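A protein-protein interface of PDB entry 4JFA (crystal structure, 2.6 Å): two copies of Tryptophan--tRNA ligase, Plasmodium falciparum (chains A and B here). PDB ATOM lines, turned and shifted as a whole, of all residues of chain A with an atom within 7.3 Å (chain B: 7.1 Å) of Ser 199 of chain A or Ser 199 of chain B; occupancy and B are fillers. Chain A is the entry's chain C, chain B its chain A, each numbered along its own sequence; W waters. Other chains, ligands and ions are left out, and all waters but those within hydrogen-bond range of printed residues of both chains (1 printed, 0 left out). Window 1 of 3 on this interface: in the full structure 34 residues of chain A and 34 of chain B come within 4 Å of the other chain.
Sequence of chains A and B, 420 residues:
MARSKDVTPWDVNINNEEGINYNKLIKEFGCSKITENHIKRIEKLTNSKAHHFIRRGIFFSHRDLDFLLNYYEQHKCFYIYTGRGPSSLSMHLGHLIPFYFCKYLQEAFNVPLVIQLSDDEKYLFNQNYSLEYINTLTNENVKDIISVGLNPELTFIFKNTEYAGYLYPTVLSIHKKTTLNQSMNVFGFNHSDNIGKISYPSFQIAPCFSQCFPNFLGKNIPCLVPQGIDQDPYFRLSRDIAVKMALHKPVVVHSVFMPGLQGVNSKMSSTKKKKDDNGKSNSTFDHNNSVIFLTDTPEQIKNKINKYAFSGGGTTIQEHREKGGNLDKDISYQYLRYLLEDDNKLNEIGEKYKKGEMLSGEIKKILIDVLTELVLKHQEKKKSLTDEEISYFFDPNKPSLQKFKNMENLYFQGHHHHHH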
ATOM      1  N   ASP A 120       3.896 -13.813  -4.257  1.00  0.00           N
ATOM      2  CA  ASP A 120       2.481 -13.764  -3.917  1.00  0.00           C
ATOM      3  C   ASP A 120       1.676 -14.734  -4.783  1.00  0.00           C
ATOM      4  O   ASP A 120       0.824 -15.464  -4.278  1.00  0.00           O
ATOM      5  CB  ASP A 120       1.945 -12.336  -4.054  1.00  0.00           C
ATOM      6  CG  ASP A 120       2.176 -11.755  -5.436  1.00  0.00           C
ATOM      7  OD1 ASP A 120       2.956 -12.345  -6.213  1.00  0.00           O
ATOM      8  OD2 ASP A 120       1.581 -10.702  -5.746  1.00  0.00           O
ATOM      9  N   LEU A 124      -0.328 -18.031  -3.583  1.00  0.00           N
ATOM     10  CA  LEU A 124      -1.774 -18.102  -3.776  1.00  0.00           C
ATOM     11  C   LEU A 124      -2.221 -19.316  -4.590  1.00  0.00           C
ATOM     12  O   LEU A 124      -3.323 -19.833  -4.392  1.00  0.00           O
ATOM     13  CB  LEU A 124      -2.277 -16.817  -4.440  1.00  0.00           C
ATOM     14  CG  LEU A 124      -2.219 -15.538  -3.603  1.00  0.00           C
ATOM     15  CD1 LEU A 124      -2.363 -14.306  -4.487  1.00  0.00           C
ATOM     16  CD2 LEU A 124      -3.293 -15.557  -2.529  1.00  0.00           C
ATOM     17  N   TYR A 168       0.569  -0.621  -5.759  1.00  0.00           N
ATOM     18  CA  TYR A 168      -0.865  -0.681  -5.451  1.00  0.00           C
ATOM     19  C   TYR A 168      -1.805   0.307  -6.166  1.00  0.00           C
ATOM     20  O   TYR A 168      -2.846  -0.116  -6.675  1.00  0.00           O
ATOM     21  CB  TYR A 168      -1.101  -0.674  -3.933  1.00  0.00           C
ATOM     22  CG  TYR A 168      -2.489  -1.108  -3.523  1.00  0.00           C
ATOM     23  CD1 TYR A 168      -2.966  -2.371  -3.845  1.00  0.00           C
ATOM     24  CD2 TYR A 168      -3.317  -0.263  -2.802  1.00  0.00           C
ATOM     25  CE1 TYR A 168      -4.235  -2.776  -3.470  1.00  0.00           C
ATOM     26  CE2 TYR A 168      -4.586  -0.660  -2.418  1.00  0.00           C
ATOM     27  CZ  TYR A 168      -5.039  -1.916  -2.755  1.00  0.00           C
ATOM     28  OH  TYR A 168      -6.301  -2.313  -2.376  1.00  0.00           O
ATOM     29  N   VAL A 171      -2.229  -0.945  -9.546  1.00  0.00           N
ATOM     30  CA  VAL A 171      -2.999  -2.183  -9.477  1.00  0.00           C
ATOM     31  C   VAL A 171      -4.495  -1.897  -9.330  1.00  0.00           C
ATOM     32  O   VAL A 171      -5.326  -2.567  -9.947  1.00  0.00           O
ATOM     33  CB  VAL A 171      -2.499  -3.082  -8.321  1.00  0.00           C
ATOM     34  CG1 VAL A 171      -3.520  -4.154  -7.974  1.00  0.00           C
ATOM     35  CG2 VAL A 171      -1.162  -3.718  -8.685  1.00  0.00           C
ATOM     36  N   HIS A 175      -7.388  -3.117 -11.593  1.00  0.00           N
ATOM     37  CA  HIS A 175      -8.477  -3.841 -10.948  1.00  0.00           C
ATOM     38  C   HIS A 175      -9.825  -3.313 -11.420  1.00  0.00           C
ATOM     39  O   HIS A 175     -10.703  -4.083 -11.808  1.00  0.00           O
ATOM     40  CB  HIS A 175      -8.385  -3.683  -9.429  1.00  0.00           C
ATOM     41  CG  HIS A 175      -7.525  -4.706  -8.758  1.00  0.00           C
ATOM     42  ND1 HIS A 175      -7.028  -5.813  -9.412  1.00  0.00           N
ATOM     43  CD2 HIS A 175      -7.079  -4.795  -7.482  1.00  0.00           C
ATOM     44  CE1 HIS A 175      -6.312  -6.536  -8.571  1.00  0.00           C
ATOM     45  NE2 HIS A 175      -6.327  -5.940  -7.393  1.00  0.00           N
ATOM     46  N   SER A 183     -11.437 -11.633 -16.082  1.00  0.00           N
ATOM     47  CA  SER A 183     -10.402 -12.359 -15.358  1.00  0.00           C
ATOM     48  C   SER A 183     -10.602 -13.863 -15.512  1.00  0.00           C
ATOM     49  O   SER A 183      -9.665 -14.595 -15.857  1.00  0.00           O
ATOM     50  CB  SER A 183     -10.419 -11.967 -13.878  1.00  0.00           C
ATOM     51  OG  SER A 183      -9.340 -12.557 -13.174  1.00  0.00           O
ATOM     52  N   PHE A 189     -10.151 -19.180 -14.558  1.00  0.00           N
ATOM     53  CA  PHE A 189     -10.469 -19.330 -13.142  1.00  0.00           C
ATOM     54  C   PHE A 189     -11.866 -19.908 -12.955  1.00  0.00           C
ATOM     55  O   PHE A 189     -12.748 -19.700 -13.793  1.00  0.00           O
ATOM     56  CB  PHE A 189     -10.393 -17.976 -12.436  1.00  0.00           C
ATOM     57  CG  PHE A 189      -9.016 -17.377 -12.410  1.00  0.00           C
ATOM     58  CD1 PHE A 189      -7.889 -18.183 -12.292  1.00  0.00           C
ATOM     59  CD2 PHE A 189      -8.845 -16.004 -12.499  1.00  0.00           C
ATOM     60  CE1 PHE A 189      -6.620 -17.626 -12.266  1.00  0.00           C
ATOM     61  CE2 PHE A 189      -7.579 -15.442 -12.473  1.00  0.00           C
ATOM     62  CZ  PHE A 189      -6.466 -16.254 -12.356  1.00  0.00           C
ATOM     63  N   ASN A 194      -9.329 -19.158  -5.061  1.00  0.00           N
ATOM     64  CA  ASN A 194      -9.327 -18.059  -4.099  1.00  0.00           C
ATOM     65  C   ASN A 194      -9.199 -16.700  -4.784  1.00  0.00           C
ATOM     66  O   ASN A 194      -8.643 -16.592  -5.880  1.00  0.00           O
ATOM     67  CB  ASN A 194      -8.243 -18.245  -3.032  1.00  0.00           C
ATOM     68  CG  ASN A 194      -6.837 -18.180  -3.601  1.00  0.00           C
ATOM     69  OD1 ASN A 194      -6.316 -17.099  -3.876  1.00  0.00           O
ATOM     70  ND2 ASN A 194      -6.206 -19.337  -3.755  1.00  0.00           N
ATOM     71  N   ILE A 195      -9.719 -15.666  -4.129  1.00  0.00           N
ATOM     72  CA  ILE A 195      -9.753 -14.319  -4.693  1.00  0.00           C
ATOM     73  C   ILE A 195      -8.358 -13.737  -4.923  1.00  0.00           C
ATOM     74  O   ILE A 195      -8.198 -12.758  -5.659  1.00  0.00           O
ATOM     75  CB  ILE A 195     -10.570 -13.369  -3.802  1.00  0.00           C
ATOM     76  CG1 ILE A 195      -9.961 -13.287  -2.400  1.00  0.00           C
ATOM     77  CG2 ILE A 195     -12.017 -13.838  -3.720  1.00  0.00           C
ATOM     78  CD1 ILE A 195     -10.790 -12.473  -1.426  1.00  0.00           C
ATOM     79  N   GLY A 196      -7.355 -14.338  -4.291  1.00  0.00           N
ATOM     80  CA  GLY A 196      -5.978 -13.944  -4.518  1.00  0.00           C
ATOM     81  C   GLY A 196      -5.533 -14.304  -5.923  1.00  0.00           C
ATOM     82  O   GLY A 196      -4.821 -13.534  -6.575  1.00  0.00           O
ATOM     83  N   LYS A 197      -5.954 -15.478  -6.390  1.00  0.00           N
ATOM     84  CA  LYS A 197      -5.641 -15.928  -7.743  1.00  0.00           C
ATOM     85  C   LYS A 197      -6.318 -15.025  -8.772  1.00  0.00           C
ATOM     86  O   LYS A 197      -5.735 -14.697  -9.806  1.00  0.00           O
ATOM     87  CB  LYS A 197      -6.072 -17.388  -7.936  1.00  0.00           C
ATOM     88  CG  LYS A 197      -5.276 -18.383  -7.099  1.00  0.00           C
ATOM     89  CD  LYS A 197      -5.987 -19.732  -6.954  1.00  0.00           C
ATOM     90  CE  LYS A 197      -5.793 -20.630  -8.162  1.00  0.00           C
ATOM     91  NZ  LYS A 197      -6.030 -22.065  -7.824  1.00  0.00           N
ATOM     92  N   ILE A 198      -7.548 -14.616  -8.471  1.00  0.00           N
ATOM     93  CA  ILE A 198      -8.302 -13.722  -9.343  1.00  0.00           C
ATOM     94  C   ILE A 198      -7.683 -12.323  -9.393  1.00  0.00           C
ATOM     95  O   ILE A 198      -7.595 -11.713 -10.460  1.00  0.00           O
ATOM     96  CB  ILE A 198      -9.788 -13.643  -8.909  1.00  0.00           C
ATOM     97  CG1 ILE A 198     -10.549 -14.883  -9.390  1.00  0.00           C
ATOM     98  CG2 ILE A 198     -10.461 -12.398  -9.458  1.00  0.00           C
ATOM     99  CD1 ILE A 198     -11.015 -15.792  -8.278  1.00  0.00           C
ATOM    100  N   SER A 199      -7.235 -11.833  -8.241  1.00  0.00           N
ATOM    101  CA  SER A 199      -6.697 -10.478  -8.141  1.00  0.00           C
ATOM    102  C   SER A 199      -5.244 -10.355  -8.601  1.00  0.00           C
ATOM    103  O   SER A 199      -4.805  -9.265  -8.964  1.00  0.00           O
ATOM    104  CB  SER A 199      -6.818  -9.962  -6.706  1.00  0.00           C
ATOM    105  OG  SER A 199      -5.684 -10.322  -5.939  1.00  0.00           O
ATOM    106  N   TYR A 200      -4.501 -11.459  -8.579  1.00  0.00           N
ATOM    107  CA  TYR A 200      -3.072 -11.421  -8.917  1.00  0.00           C
ATOM    108  C   TYR A 200      -2.670 -10.768 -10.254  1.00  0.00           C
ATOM    109  O   TYR A 200      -1.743  -9.954 -10.269  1.00  0.00           O
ATOM    110  CB  TYR A 200      -2.406 -12.800  -8.805  1.00  0.00           C
ATOM    111  CG  TYR A 200      -1.041 -12.808  -9.457  1.00  0.00           C
ATOM    112  CD1 TYR A 200      -0.837 -13.423 -10.684  1.00  0.00           C
ATOM    113  CD2 TYR A 200       0.032 -12.154  -8.868  1.00  0.00           C
ATOM    114  CE1 TYR A 200       0.405 -13.406 -11.295  1.00  0.00           C
ATOM    115  CE2 TYR A 200       1.276 -12.133  -9.471  1.00  0.00           C
ATOM    116  CZ  TYR A 200       1.455 -12.762 -10.683  1.00  0.00           C
ATOM    117  OH  TYR A 200       2.690 -12.744 -11.287  1.00  0.00           O
ATOM    118  N   PRO A 201      -3.332 -11.140 -11.374  1.00  0.00           N
ATOM    119  CA  PRO A 201      -2.867 -10.664 -12.687  1.00  0.00           C
ATOM    120  C   PRO A 201      -2.638  -9.153 -12.796  1.00  0.00           C
ATOM    121  O   PRO A 201      -1.813  -8.736 -13.608  1.00  0.00           O
ATOM    122  CB  PRO A 201      -3.998 -11.088 -13.626  1.00  0.00           C
ATOM    123  CG  PRO A 201      -4.545 -12.317 -13.000  1.00  0.00           C
ATOM    124  CD  PRO A 201      -4.482 -12.058 -11.515  1.00  0.00           C
ATOM    125  N   SER A 202      -3.344  -8.357 -11.999  1.00  0.00           N
ATOM    126  CA  SER A 202      -3.130  -6.916 -11.998  1.00  0.00           C
ATOM    127  C   SER A 202      -1.737  -6.571 -11.479  1.00  0.00           C
ATOM    128  O   SER A 202      -1.139  -5.576 -11.894  1.00  0.00           O
ATOM    129  CB  SER A 202      -4.192  -6.217 -11.154  1.00  0.00           C
ATOM    130  OG  SER A 202      -5.494  -6.498 -11.638  1.00  0.00           O
ATOM    131  N   PHE A 203      -1.223  -7.398 -10.573  1.00  0.00           N
ATOM    132  CA  PHE A 203       0.105  -7.185 -10.009  1.00  0.00           C
ATOM    133  C   PHE A 203       1.205  -7.550 -10.999  1.00  0.00           C
ATOM    134  O   PHE A 203       2.295  -6.982 -10.957  1.00  0.00           O
ATOM    135  CB  PHE A 203       0.269  -7.978  -8.712  1.00  0.00           C
ATOM    136  CG  PHE A 203      -0.489  -7.400  -7.551  1.00  0.00           C
ATOM    137  CD1 PHE A 203       0.135  -6.536  -6.662  1.00  0.00           C
ATOM    138  CD2 PHE A 203      -1.825  -7.717  -7.345  1.00  0.00           C
ATOM    139  CE1 PHE A 203      -0.556  -5.999  -5.589  1.00  0.00           C
ATOM    140  CE2 PHE A 203      -2.523  -7.181  -6.273  1.00  0.00           C
ATOM    141  CZ  PHE A 203      -1.887  -6.322  -5.395  1.00  0.00           C
ATOM    142  N   GLN A 204       0.924  -8.498 -11.886  1.00  0.00           N
ATOM    143  CA  GLN A 204       1.875  -8.851 -12.937  1.00  0.00           C
ATOM    144  C   GLN A 204       1.830  -7.818 -14.062  1.00  0.00           C
ATOM    145  O   GLN A 204       2.831  -7.571 -14.741  1.00  0.00           O
ATOM    146  CB  GLN A 204       1.585 -10.254 -13.482  1.00  0.00           C
ATOM    147  CG  GLN A 204       2.531 -10.693 -14.595  1.00  0.00           C
ATOM    148  CD  GLN A 204       2.615 -12.199 -14.737  1.00  0.00           C
ATOM    149  OE1 GLN A 204       2.381 -12.938 -13.782  1.00  0.00           O
ATOM    150  NE2 GLN A 204       2.957 -12.662 -15.935  1.00  0.00           N
ATOM    151  N   LEU B 124     -12.807   1.881  -6.124  1.00  0.00           N
ATOM    152  CA  LEU B 124     -13.214   0.686  -6.858  1.00  0.00           C
ATOM    153  C   LEU B 124     -14.731   0.526  -6.996  1.00  0.00           C
ATOM    154  O   LEU B 124     -15.203  -0.194  -7.879  1.00  0.00           O
ATOM    155  CB  LEU B 124     -12.619  -0.562  -6.200  1.00  0.00           C
ATOM    156  CG  LEU B 124     -11.097  -0.705  -6.230  1.00  0.00           C
ATOM    157  CD1 LEU B 124     -10.638  -1.767  -5.243  1.00  0.00           C
ATOM    158  CD2 LEU B 124     -10.614  -1.034  -7.633  1.00  0.00           C
ATOM    159  N   TYR B 168      -0.143  -6.160   2.901  1.00  0.00           N
ATOM    160  CA  TYR B 168      -0.183  -7.172   1.838  1.00  0.00           C
ATOM    161  C   TYR B 168       0.047  -8.642   2.229  1.00  0.00           C
ATOM    162  O   TYR B 168      -0.727  -9.506   1.811  1.00  0.00           O
ATOM    163  CB  TYR B 168       0.715  -6.768   0.657  1.00  0.00           C
ATOM    164  CG  TYR B 168       0.395  -7.501  -0.627  1.00  0.00           C
ATOM    165  CD1 TYR B 168      -0.904  -7.553  -1.113  1.00  0.00           C
ATOM    166  CD2 TYR B 168       1.392  -8.134  -1.357  1.00  0.00           C
ATOM    167  CE1 TYR B 168      -1.203  -8.219  -2.285  1.00  0.00           C
ATOM    168  CE2 TYR B 168       1.102  -8.798  -2.535  1.00  0.00           C
ATOM    169  CZ  TYR B 168      -0.197  -8.840  -2.993  1.00  0.00           C
ATOM    170  OH  TYR B 168      -0.488  -9.503  -4.161  1.00  0.00           O
ATOM    171  N   VAL B 171      -3.039  -9.775   3.887  1.00  0.00           N
ATOM    172  CA  VAL B 171      -4.120  -9.804   2.904  1.00  0.00           C
ATOM    173  C   VAL B 171      -4.014 -11.051   2.026  1.00  0.00           C
ATOM    174  O   VAL B 171      -5.025 -11.663   1.678  1.00  0.00           O
ATOM    175  CB  VAL B 171      -4.109  -8.528   2.035  1.00  0.00           C
ATOM    176  CG1 VAL B 171      -4.987  -8.694   0.803  1.00  0.00           C
ATOM    177  CG2 VAL B 171      -4.565  -7.328   2.852  1.00  0.00           C
ATOM    178  N   LEU B 172      -2.781 -11.427   1.689  1.00  0.00           N
ATOM    179  CA  LEU B 172      -2.517 -12.617   0.884  1.00  0.00           C
ATOM    180  C   LEU B 172      -3.020 -13.889   1.565  1.00  0.00           C
ATOM    181  O   LEU B 172      -3.607 -14.757   0.917  1.00  0.00           O
ATOM    182  CB  LEU B 172      -1.020 -12.738   0.593  1.00  0.00           C
ATOM    183  CG  LEU B 172      -0.438 -11.808  -0.474  1.00  0.00           C
ATOM    184  CD1 LEU B 172       1.082 -11.867  -0.472  1.00  0.00           C
ATOM    185  CD2 LEU B 172      -0.976 -12.180  -1.843  1.00  0.00           C
ATOM    186  N   HIS B 175      -6.753 -13.682   1.461  1.00  0.00           N
ATOM    187  CA  HIS B 175      -7.133 -13.979   0.084  1.00  0.00           C
ATOM    188  C   HIS B 175      -7.198 -15.484  -0.137  1.00  0.00           C
ATOM    189  O   HIS B 175      -8.210 -16.018  -0.591  1.00  0.00           O
ATOM    190  CB  HIS B 175      -6.108 -13.384  -0.883  1.00  0.00           C
ATOM    191  CG  HIS B 175      -6.391 -11.969  -1.282  1.00  0.00           C
ATOM    192  ND1 HIS B 175      -7.530 -11.296  -0.899  1.00  0.00           N
ATOM    193  CD2 HIS B 175      -5.677 -11.103  -2.041  1.00  0.00           C
ATOM    194  CE1 HIS B 175      -7.505 -10.073  -1.402  1.00  0.00           C
ATOM    195  NE2 HIS B 175      -6.393  -9.931  -2.097  1.00  0.00           N
ATOM    196  N   SER B 183     -16.766 -15.151  -1.457  1.00  0.00           N
ATOM    197  CA  SER B 183     -16.734 -13.696  -1.555  1.00  0.00           C
ATOM    198  C   SER B 183     -18.019 -13.168  -2.190  1.00  0.00           C
ATOM    199  O   SER B 183     -18.657 -12.251  -1.658  1.00  0.00           O
ATOM    200  CB  SER B 183     -15.516 -13.246  -2.363  1.00  0.00           C
ATOM    201  OG  SER B 183     -15.410 -11.835  -2.388  1.00  0.00           O
ATOM    202  N   PHE B 189     -21.673 -10.001  -4.816  1.00  0.00           N
ATOM    203  CA  PHE B 189     -21.028  -9.580  -6.052  1.00  0.00           C
ATOM    204  C   PHE B 189     -21.601 -10.339  -7.240  1.00  0.00           C
ATOM    205  O   PHE B 189     -22.079 -11.468  -7.095  1.00  0.00           O
ATOM    206  CB  PHE B 189     -19.523  -9.833  -5.979  1.00  0.00           C
ATOM    207  CG  PHE B 189     -18.812  -8.993  -4.959  1.00  0.00           C
ATOM    208  CD1 PHE B 189     -19.100  -7.641  -4.823  1.00  0.00           C
ATOM    209  CD2 PHE B 189     -17.851  -9.556  -4.133  1.00  0.00           C
ATOM    210  CE1 PHE B 189     -18.440  -6.868  -3.880  1.00  0.00           C
ATOM    211  CE2 PHE B 189     -17.189  -8.790  -3.188  1.00  0.00           C
ATOM    212  CZ  PHE B 189     -17.485  -7.446  -3.060  1.00  0.00           C
ATOM    213  N   ASN B 194     -15.883  -5.400 -10.992  1.00  0.00           N
ATOM    214  CA  ASN B 194     -14.443  -5.495 -11.197  1.00  0.00           C
ATOM    215  C   ASN B 194     -13.783  -6.319 -10.095  1.00  0.00           C
ATOM    216  O   ASN B 194     -14.345  -6.481  -9.009  1.00  0.00           O
ATOM    217  CB  ASN B 194     -13.804  -4.108 -11.310  1.00  0.00           C
ATOM    218  CG  ASN B 194     -13.921  -3.301 -10.032  1.00  0.00           C
ATOM    219  OD1 ASN B 194     -13.209  -3.550  -9.058  1.00  0.00           O
ATOM    220  ND2 ASN B 194     -14.803  -2.308 -10.037  1.00  0.00           N
ATOM    221  N   ILE B 195     -12.594  -6.841 -10.379  1.00  0.00           N
ATOM    222  CA  ILE B 195     -11.910  -7.727  -9.444  1.00  0.00           C
ATOM    223  C   ILE B 195     -11.385  -6.994  -8.210  1.00  0.00           C
ATOM    224  O   ILE B 195     -11.039  -7.625  -7.207  1.00  0.00           O
ATOM    225  CB  ILE B 195     -10.767  -8.493 -10.135  1.00  0.00           C
ATOM    226  CG1 ILE B 195      -9.727  -7.524 -10.701  1.00  0.00           C
ATOM    227  CG2 ILE B 195     -11.321  -9.379 -11.241  1.00  0.00           C
ATOM    228  CD1 ILE B 195      -8.621  -8.212 -11.484  1.00  0.00           C
ATOM    229  N   GLY B 196     -11.331  -5.667  -8.283  1.00  0.00           N
ATOM    230  CA  GLY B 196     -10.910  -4.861  -7.153  1.00  0.00           C
ATOM    231  C   GLY B 196     -11.932  -4.887  -6.035  1.00  0.00           C
ATOM    232  O   GLY B 196     -11.569  -4.881  -4.853  1.00  0.00           O
ATOM    233  N   LYS B 197     -13.211  -4.919  -6.406  1.00  0.00           N
ATOM    234  CA  LYS B 197     -14.303  -4.984  -5.433  1.00  0.00           C
ATOM    235  C   LYS B 197     -14.307  -6.346  -4.737  1.00  0.00           C
ATOM    236  O   LYS B 197     -14.597  -6.447  -3.542  1.00  0.00           O
ATOM    237  CB  LYS B 197     -15.644  -4.727  -6.133  1.00  0.00           C
ATOM    238  CG  LYS B 197     -15.794  -3.315  -6.693  1.00  0.00           C
ATOM    239  CD  LYS B 197     -16.886  -3.225  -7.766  1.00  0.00           C
ATOM    240  CE  LYS B 197     -18.286  -3.262  -7.182  1.00  0.00           C
ATOM    241  NZ  LYS B 197     -19.289  -2.544  -8.030  1.00  0.00           N
ATOM    242  N   ILE B 198     -13.963  -7.386  -5.492  1.00  0.00           N
ATOM    243  CA  ILE B 198     -13.891  -8.747  -4.963  1.00  0.00           C
ATOM    244  C   ILE B 198     -12.658  -8.907  -4.073  1.00  0.00           C
ATOM    245  O   ILE B 198     -12.678  -9.639  -3.080  1.00  0.00           O
ATOM    246  CB  ILE B 198     -13.903  -9.777  -6.121  1.00  0.00           C
ATOM    247  CG1 ILE B 198     -15.323  -9.904  -6.676  1.00  0.00           C
ATOM    248  CG2 ILE B 198     -13.386 -11.132  -5.683  1.00  0.00           C
ATOM    249  CD1 ILE B 198     -15.386 -10.126  -8.162  1.00  0.00           C
ATOM    250  N   SER B 199     -11.601  -8.178  -4.413  1.00  0.00           N
ATOM    251  CA  SER B 199     -10.365  -8.189  -3.641  1.00  0.00           C
ATOM    252  C   SER B 199     -10.503  -7.445  -2.316  1.00  0.00           C
ATOM    253  O   SER B 199     -10.025  -7.922  -1.287  1.00  0.00           O
ATOM    254  CB  SER B 199      -9.233  -7.555  -4.452  1.00  0.00           C
ATOM    255  OG  SER B 199      -9.148  -8.122  -5.745  1.00  0.00           O
ATOM    256  N   TYR B 200     -11.156  -6.284  -2.349  1.00  0.00           N
ATOM    257  CA  TYR B 200     -11.168  -5.351  -1.214  1.00  0.00           C
ATOM    258  C   TYR B 200     -11.406  -5.897   0.207  1.00  0.00           C
ATOM    259  O   TYR B 200     -10.663  -5.532   1.119  1.00  0.00           O
ATOM    260  CB  TYR B 200     -12.099  -4.154  -1.460  1.00  0.00           C
ATOM    261  CG  TYR B 200     -12.280  -3.336  -0.204  1.00  0.00           C
ATOM    262  CD1 TYR B 200     -13.462  -3.386   0.520  1.00  0.00           C
ATOM    263  CD2 TYR B 200     -11.245  -2.553   0.286  1.00  0.00           C
ATOM    264  CE1 TYR B 200     -13.616  -2.657   1.683  1.00  0.00           C
ATOM    265  CE2 TYR B 200     -11.390  -1.823   1.447  1.00  0.00           C
ATOM    266  CZ  TYR B 200     -12.577  -1.878   2.140  1.00  0.00           C
ATOM    267  OH  TYR B 200     -12.725  -1.153   3.298  1.00  0.00           O
ATOM    268  N   PRO B 201     -12.450  -6.733   0.409  1.00  0.00           N
ATOM    269  CA  PRO B 201     -12.796  -7.153   1.777  1.00  0.00           C
ATOM    270  C   PRO B 201     -11.618  -7.652   2.620  1.00  0.00           C
ATOM    271  O   PRO B 201     -11.615  -7.437   3.833  1.00  0.00           O
ATOM    272  CB  PRO B 201     -13.790  -8.293   1.546  1.00  0.00           C
ATOM    273  CG  PRO B 201     -14.462  -7.935   0.270  1.00  0.00           C
ATOM    274  CD  PRO B 201     -13.394  -7.294  -0.581  1.00  0.00           C
ATOM    275  N   SER B 202     -10.636  -8.290   1.989  1.00  0.00           N
ATOM    276  CA  SER B 202      -9.453  -8.761   2.701  1.00  0.00           C
ATOM    277  C   SER B 202      -8.631  -7.600   3.261  1.00  0.00           C
ATOM    278  O   SER B 202      -7.899  -7.767   4.239  1.00  0.00           O
ATOM    279  CB  SER B 202      -8.583  -9.622   1.785  1.00  0.00           C
ATOM    280  OG  SER B 202      -9.303 -10.741   1.294  1.00  0.00           O
ATOM    281  N   PHE B 203      -8.754  -6.429   2.642  1.00  0.00           N
ATOM    282  CA  PHE B 203      -8.033  -5.247   3.099  1.00  0.00           C
ATOM    283  C   PHE B 203      -8.707  -4.602   4.304  1.00  0.00           C
ATOM    284  O   PHE B 203      -8.042  -3.977   5.130  1.00  0.00           O
ATOM    285  CB  PHE B 203      -7.885  -4.228   1.966  1.00  0.00           C
ATOM    286  CG  PHE B 203      -6.897  -4.634   0.909  1.00  0.00           C
ATOM    287  CD1 PHE B 203      -5.606  -4.122   0.915  1.00  0.00           C
ATOM    288  CD2 PHE B 203      -7.256  -5.525  -0.093  1.00  0.00           C
ATOM    289  CE1 PHE B 203      -4.691  -4.492  -0.059  1.00  0.00           C
ATOM    290  CE2 PHE B 203      -6.346  -5.899  -1.071  1.00  0.00           C
ATOM    291  CZ  PHE B 203      -5.063  -5.382  -1.053  1.00  0.00           C
ATOM    292  N   GLN B 204     -10.025  -4.746   4.403  1.00  0.00           N
ATOM    293  CA  GLN B 204     -10.756  -4.243   5.562  1.00  0.00           C
ATOM    294  C   GLN B 204     -10.617  -5.217   6.732  1.00  0.00           C
ATOM    295  O   GLN B 204     -10.662  -4.824   7.901  1.00  0.00           O
ATOM    296  CB  GLN B 204     -12.233  -4.022   5.216  1.00  0.00           C
ATOM    297  CG  GLN B 204     -13.079  -3.542   6.389  1.00  0.00           C
ATOM    298  CD  GLN B 204     -14.397  -2.937   5.953  1.00  0.00           C
ATOM    299  OE1 GLN B 204     -14.489  -2.318   4.893  1.00  0.00           O
ATOM    300  NE2 GLN B 204     -15.425  -3.106   6.776  1.00  0.00           N
HETATM  301  O   HOH W   1      -3.142 -10.407  -4.896  1.00  0.00           O
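Printed residues of chain B within 4 Å of Ser 183 of chain A: Ile 195 (3.8 Å).
Ser 199 of chain A touches just these residues of chain B: His 175 (3.9 Å) and Ser 199 (3.1 Å).
Of the printed residues of chain A, Ile 195 of chain B touches His 175 (3.4 Å), Ser 183 (3.8 Å), Ile 198 (3.6 Å) and Ser 202 (3.6 Å).
Ser 199 of chain B touches just these residues of chain A: His 175 (3.9 Å) and Ser 199 (3.1 Å).
The nearest residue of chain B that does not touch Ser 199 of chain A is Ile 195 of chain B (4.5 Å).
The nearest printed residue of chain B that does not touch Asn 194 of chain A is Leu 172 of chain B (6.0 Å).
Ile 195 of chain A touches Ser 202 of chain B, and with the chains exchanged Ser 202 of chain A touches Ile 195 of chain B.
Water W1 lies within hydrogen-bond range of the side-chain hydroxyl (OG) of Ser 199 of chain A (2.7 Å) and the side-chain hydroxyl (OH) of Tyr 168 of chain B (2.9 Å).
OH of Tyr 168 of chain B sits at hydrogen-bond distance from OD2 of Asp 120 of chain A (2.9 Å).
Of the 18 printed residues of chain B, 12 touch a printed residue of chain A.
Hydrophobic or aromatic side chains of chain B that line the printed part of chain A: Leu 124, Tyr 168, Leu 172, His 175, Ile 195, Ile 198 and Phe 203.
Along chain B the printed residues that touch a printed residue of chain A span positions 124 to 203.
Of the 18 printed residues of chain A, 12 touch a printed residue of chain B.
Among the printed residues, no Asp or Glu carboxylate lies within 4 Å of a Lys or Arg side-chain nitrogen of the other chain.
OD1 of Asn 194 of chain B lies within hydrogen-bond range of N of Lys 197 of chain B, 3.0 Å away.
N of Gly 196 of chain A lies within hydrogen-bond range of OD1 of Asn 194 of chain A (3.0 Å).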
